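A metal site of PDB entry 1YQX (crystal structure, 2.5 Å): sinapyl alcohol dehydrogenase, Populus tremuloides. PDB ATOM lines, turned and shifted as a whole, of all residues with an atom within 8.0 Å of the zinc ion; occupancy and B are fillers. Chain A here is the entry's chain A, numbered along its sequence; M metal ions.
His 108 touches the zinc ion.
Within 4 Å of the zinc ion: Cys 107, His 108, Cys 110, Cys 113 and Cys 121.
SG of Cys 107 sits close to OG of Ser 109, 3.2 Å away.
N of His 108 lies close to SG of Cys 113, 3.2 Å away.
The guanidinium group (NH2) of Arg 151 lies within hydrogen-bond range of the backbone carbonyl oxygen (O) of Cys 113 (3.3 Å).
The side-chain sulfur (SG) of Cys 121 sits close to the backbone NH (N) of Lys 123.
SG of Cys 121 lies close to N of Met 124.
The side-chain sulfur of Cys 110 sits close to the backbone NH of Ser 112, at 3.2 Å.
A ring nitrogen (NE2) of His 108 is in hydrogen-bond range of the backbone NH (N) of Ala 106 (3.4 Å).
OH of Tyr 152 is in hydrogen-bond range of NE2 of His 108 (2.5 Å).
The zinc ion is bound by SG of Cys 107, SG of Cys 113, SG of Cys 121 and SG of Cys 110.
The zinc ion has four donor atoms within binding distance.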
ATOM      1  N   GLY A 105     -22.965   3.264  10.679  1.00  0.00           N
ATOM      2  CA  GLY A 105     -22.981   1.960  11.316  1.00  0.00           C
ATOM      3  C   GLY A 105     -22.911   2.022  12.828  1.00  0.00           C
ATOM      4  O   GLY A 105     -22.565   3.046  13.404  1.00  0.00           O
ATOM      5  N   ALA A 106     -23.266   0.921  13.483  1.00  0.00           N
ATOM      6  CA  ALA A 106     -23.236   0.831  14.943  1.00  0.00           C
ATOM      7  C   ALA A 106     -23.193  -0.662  15.336  1.00  0.00           C
ATOM      8  O   ALA A 106     -23.122  -1.523  14.452  1.00  0.00           O
ATOM      9  CB  ALA A 106     -24.477   1.501  15.544  1.00  0.00           C
ATOM     10  N   CYS A 107     -23.229  -0.970  16.633  1.00  0.00           N
ATOM     11  CA  CYS A 107     -23.174  -2.362  17.052  1.00  0.00           C
ATOM     12  C   CYS A 107     -24.490  -3.098  16.749  1.00  0.00           C
ATOM     13  O   CYS A 107     -24.481  -4.297  16.454  1.00  0.00           O
ATOM     14  CB  CYS A 107     -22.819  -2.485  18.537  1.00  0.00           C
ATOM     15  SG  CYS A 107     -24.201  -2.426  19.707  1.00  0.00           S
ATOM     16  N   HIS A 108     -25.601  -2.387  16.803  1.00  0.00           N
ATOM     17  CA  HIS A 108     -26.923  -2.968  16.518  1.00  0.00           C
ATOM     18  C   HIS A 108     -27.280  -4.097  17.491  1.00  0.00           C
ATOM     19  O   HIS A 108     -27.624  -5.200  17.060  1.00  0.00           O
ATOM     20  CB  HIS A 108     -26.986  -3.508  15.082  1.00  0.00           C
ATOM     21  CG  HIS A 108     -26.707  -2.478  14.018  1.00  0.00           C
ATOM     22  ND1 HIS A 108     -26.884  -2.737  12.681  1.00  0.00           N
ATOM     23  CD2 HIS A 108     -26.258  -1.199  14.098  1.00  0.00           C
ATOM     24  CE1 HIS A 108     -26.554  -1.666  11.976  1.00  0.00           C
ATOM     25  NE2 HIS A 108     -26.167  -0.722  12.810  1.00  0.00           N
ATOM     26  N   SER A 109     -27.197  -3.829  18.788  1.00  0.00           N
ATOM     27  CA  SER A 109     -27.527  -4.843  19.780  1.00  0.00           C
ATOM     28  C   SER A 109     -27.674  -4.290  21.191  1.00  0.00           C
ATOM     29  O   SER A 109     -28.348  -4.889  22.034  1.00  0.00           O
ATOM     30  CB  SER A 109     -26.483  -5.957  19.764  1.00  0.00           C
ATOM     31  OG  SER A 109     -25.197  -5.430  19.986  1.00  0.00           O
ATOM     32  N   CYS A 110     -27.046  -3.149  21.471  1.00  0.00           N
ATOM     33  CA  CYS A 110     -27.168  -2.549  22.794  1.00  0.00           C
ATOM     34  C   CYS A 110     -28.583  -1.972  22.878  1.00  0.00           C
ATOM     35  O   CYS A 110     -29.371  -2.155  21.958  1.00  0.00           O
ATOM     36  CB  CYS A 110     -26.147  -1.431  22.985  1.00  0.00           C
ATOM     37  SG  CYS A 110     -26.460  -0.007  21.947  1.00  0.00           S
ATOM     38  N   GLU A 111     -28.908  -1.293  23.969  1.00  0.00           N
ATOM     39  CA  GLU A 111     -30.257  -0.734  24.070  1.00  0.00           C
ATOM     40  C   GLU A 111     -30.403   0.585  23.319  1.00  0.00           C
ATOM     41  O   GLU A 111     -31.524   1.053  23.077  1.00  0.00           O
ATOM     42  CB  GLU A 111     -30.658  -0.535  25.535  1.00  0.00           C
ATOM     43  CG  GLU A 111     -32.164  -0.679  25.725  1.00  0.00           C
ATOM     44  CD  GLU A 111     -32.625  -0.429  27.155  1.00  0.00           C
ATOM     45  OE1 GLU A 111     -32.857   0.755  27.498  1.00  0.00           O
ATOM     46  OE2 GLU A 111     -32.738  -1.404  27.931  1.00  0.00           O
ATOM     47  N   SER A 112     -29.287   1.187  22.949  1.00  0.00           N
ATOM     48  CA  SER A 112     -29.321   2.446  22.210  1.00  0.00           C
ATOM     49  C   SER A 112     -29.832   2.180  20.801  1.00  0.00           C
ATOM     50  O   SER A 112     -30.705   2.884  20.302  1.00  0.00           O
ATOM     51  CB  SER A 112     -27.924   3.049  22.150  1.00  0.00           C
ATOM     52  OG  SER A 112     -27.972   4.406  21.743  1.00  0.00           O
ATOM     53  N   CYS A 113     -29.300   1.141  20.174  1.00  0.00           N
ATOM     54  CA  CYS A 113     -29.696   0.761  18.826  1.00  0.00           C
ATOM     55  C   CYS A 113     -31.157   0.311  18.747  1.00  0.00           C
ATOM     56  O   CYS A 113     -31.915   0.778  17.880  1.00  0.00           O
ATOM     57  CB  CYS A 113     -28.787  -0.352  18.294  1.00  0.00           C
ATOM     58  SG  CYS A 113     -27.110   0.199  17.999  1.00  0.00           S
ATOM     59  N   ALA A 114     -31.544  -0.589  19.635  1.00  0.00           N
ATOM     60  CA  ALA A 114     -32.915  -1.091  19.679  1.00  0.00           C
ATOM     61  C   ALA A 114     -33.913   0.054  19.826  1.00  0.00           C
ATOM     62  O   ALA A 114     -35.021   0.004  19.270  1.00  0.00           O
ATOM     63  CB  ALA A 114     -33.073  -2.080  20.845  1.00  0.00           C
ATOM     64  N   LEU A 117     -31.313   4.737  18.438  1.00  0.00           N
ATOM     65  CA  LEU A 117     -30.361   5.786  18.729  1.00  0.00           C
ATOM     66  C   LEU A 117     -28.955   5.332  18.394  1.00  0.00           C
ATOM     67  O   LEU A 117     -28.056   5.405  19.217  1.00  0.00           O
ATOM     68  CB  LEU A 117     -30.454   6.192  20.198  1.00  0.00           C
ATOM     69  CG  LEU A 117     -31.784   6.833  20.621  1.00  0.00           C
ATOM     70  CD1 LEU A 117     -31.827   6.956  22.135  1.00  0.00           C
ATOM     71  CD2 LEU A 117     -31.938   8.201  19.943  1.00  0.00           C
ATOM     72  N   GLU A 118     -28.771   4.862  17.164  1.00  0.00           N
ATOM     73  CA  GLU A 118     -27.454   4.415  16.725  1.00  0.00           C
ATOM     74  C   GLU A 118     -26.424   5.484  17.029  1.00  0.00           C
ATOM     75  O   GLU A 118     -25.236   5.197  17.174  1.00  0.00           O
ATOM     76  CB  GLU A 118     -27.457   4.123  15.225  1.00  0.00           C
ATOM     77  CG  GLU A 118     -28.484   3.102  14.765  1.00  0.00           C
ATOM     78  CD  GLU A 118     -29.877   3.686  14.585  1.00  0.00           C
ATOM     79  OE1 GLU A 118     -30.791   2.933  14.194  1.00  0.00           O
ATOM     80  OE2 GLU A 118     -30.066   4.907  14.815  1.00  0.00           O
ATOM     81  N   ASN A 119     -26.884   6.733  17.139  1.00  0.00           N
ATOM     82  CA  ASN A 119     -25.983   7.857  17.409  1.00  0.00           C
ATOM     83  C   ASN A 119     -25.454   7.859  18.836  1.00  0.00           C
ATOM     84  O   ASN A 119     -24.472   8.560  19.133  1.00  0.00           O
ATOM     85  CB  ASN A 119     -26.678   9.199  17.095  1.00  0.00           C
ATOM     86  CG  ASN A 119     -27.974   9.409  17.878  1.00  0.00           C
ATOM     87  OD1 ASN A 119     -28.772   8.496  18.040  1.00  0.00           O
ATOM     88  ND2 ASN A 119     -28.181  10.642  18.333  1.00  0.00           N
ATOM     89  N   TYR A 120     -26.068   7.085  19.705  1.00  0.00           N
ATOM     90  CA  TYR A 120     -25.606   7.027  21.088  1.00  0.00           C
ATOM     91  C   TYR A 120     -25.058   5.655  21.453  1.00  0.00           C
ATOM     92  O   TYR A 120     -24.933   5.316  22.628  1.00  0.00           O
ATOM     93  CB  TYR A 120     -26.734   7.414  22.049  1.00  0.00           C
ATOM     94  CG  TYR A 120     -27.134   8.867  21.928  1.00  0.00           C
ATOM     95  CD1 TYR A 120     -28.443   9.227  21.597  1.00  0.00           C
ATOM     96  CD2 TYR A 120     -26.191   9.878  22.122  1.00  0.00           C
ATOM     97  CE1 TYR A 120     -28.803  10.567  21.450  1.00  0.00           C
ATOM     98  CE2 TYR A 120     -26.540  11.218  21.984  1.00  0.00           C
ATOM     99  CZ  TYR A 120     -27.838  11.559  21.649  1.00  0.00           C
ATOM    100  OH  TYR A 120     -28.175  12.878  21.493  1.00  0.00           O
ATOM    101  N   CYS A 121     -24.724   4.871  20.425  1.00  0.00           N
ATOM    102  CA  CYS A 121     -24.145   3.543  20.624  1.00  0.00           C
ATOM    103  C   CYS A 121     -22.664   3.726  20.928  1.00  0.00           C
ATOM    104  O   CYS A 121     -21.987   4.531  20.284  1.00  0.00           O
ATOM    105  CB  CYS A 121     -24.298   2.691  19.355  1.00  0.00           C
ATOM    106  SG  CYS A 121     -23.269   1.186  19.331  1.00  0.00           S
ATOM    107  N   PRO A 122     -22.147   2.979  21.907  1.00  0.00           N
ATOM    108  CA  PRO A 122     -20.719   3.135  22.222  1.00  0.00           C
ATOM    109  C   PRO A 122     -19.803   2.715  21.069  1.00  0.00           C
ATOM    110  O   PRO A 122     -18.632   3.080  21.046  1.00  0.00           O
ATOM    111  CB  PRO A 122     -20.542   2.294  23.481  1.00  0.00           C
ATOM    112  CG  PRO A 122     -21.620   1.252  23.347  1.00  0.00           C
ATOM    113  CD  PRO A 122     -22.785   2.033  22.842  1.00  0.00           C
ATOM    114  N   LYS A 123     -20.366   1.979  20.107  1.00  0.00           N
ATOM    115  CA  LYS A 123     -19.596   1.513  18.957  1.00  0.00           C
ATOM    116  C   LYS A 123     -20.108   2.135  17.656  1.00  0.00           C
ATOM    117  O   LYS A 123     -19.883   1.597  16.567  1.00  0.00           O
ATOM    118  CB  LYS A 123     -19.658  -0.010  18.840  1.00  0.00           C
ATOM    119  CG  LYS A 123     -19.159  -0.790  20.064  1.00  0.00           C
ATOM    120  CD  LYS A 123     -19.470  -2.270  19.893  1.00  0.00           C
ATOM    121  CE  LYS A 123     -19.274  -3.064  21.178  1.00  0.00           C
ATOM    122  NZ  LYS A 123     -19.756  -4.482  21.002  1.00  0.00           N
ATOM    123  N   MET A 124     -20.815   3.251  17.767  1.00  0.00           N
ATOM    124  CA  MET A 124     -21.343   3.933  16.586  1.00  0.00           C
ATOM    125  C   MET A 124     -20.185   4.302  15.673  1.00  0.00           C
ATOM    126  O   MET A 124     -19.131   4.707  16.148  1.00  0.00           O
ATOM    127  CB  MET A 124     -22.101   5.196  16.997  1.00  0.00           C
ATOM    128  CG  MET A 124     -21.289   6.133  17.879  1.00  0.00           C
ATOM    129  SD  MET A 124     -21.208   7.817  17.264  1.00  0.00           S
ATOM    130  CE  MET A 124     -19.460   8.034  17.122  1.00  0.00           C
ATOM    131  N   ARG A 151     -29.900   0.734   6.313  1.00  0.00           N
ATOM    132  CA  ARG A 151     -30.330   1.315   7.596  1.00  0.00           C
ATOM    133  C   ARG A 151     -29.810   2.744   7.804  1.00  0.00           C
ATOM    134  O   ARG A 151     -30.363   3.493   8.603  1.00  0.00           O
ATOM    135  CB  ARG A 151     -29.864   0.435   8.763  1.00  0.00           C
ATOM    136  CG  ARG A 151     -30.211   0.981  10.145  1.00  0.00           C
ATOM    137  CD  ARG A 151     -29.900  -0.029  11.274  1.00  0.00           C
ATOM    138  NE  ARG A 151     -30.208   0.513  12.603  1.00  0.00           N
ATOM    139  CZ  ARG A 151     -30.250  -0.204  13.717  1.00  0.00           C
ATOM    140  NH1 ARG A 151     -30.014  -1.511  13.688  1.00  0.00           N
ATOM    141  NH2 ARG A 151     -30.548   0.378  14.871  1.00  0.00           N
ATOM    142  N   TYR A 152     -28.759   3.103   7.080  1.00  0.00           N
ATOM    143  CA  TYR A 152     -28.194   4.436   7.210  1.00  0.00           C
ATOM    144  C   TYR A 152     -28.428   5.274   5.967  1.00  0.00           C
ATOM    145  O   TYR A 152     -27.852   6.343   5.805  1.00  0.00           O
ATOM    146  CB  TYR A 152     -26.701   4.345   7.539  1.00  0.00           C
ATOM    147  CG  TYR A 152     -26.486   3.639   8.852  1.00  0.00           C
ATOM    148  CD1 TYR A 152     -26.459   2.246   8.931  1.00  0.00           C
ATOM    149  CD2 TYR A 152     -26.398   4.368  10.033  1.00  0.00           C
ATOM    150  CE1 TYR A 152     -26.370   1.612  10.157  1.00  0.00           C
ATOM    151  CE2 TYR A 152     -26.309   3.734  11.259  1.00  0.00           C
ATOM    152  CZ  TYR A 152     -26.293   2.364  11.320  1.00  0.00           C
ATOM    153  OH  TYR A 152     -26.202   1.747  12.545  1.00  0.00           O
HETATM  154 ZN    ZN M   1     -25.277  -0.337  19.539  1.00  0.00          ZN
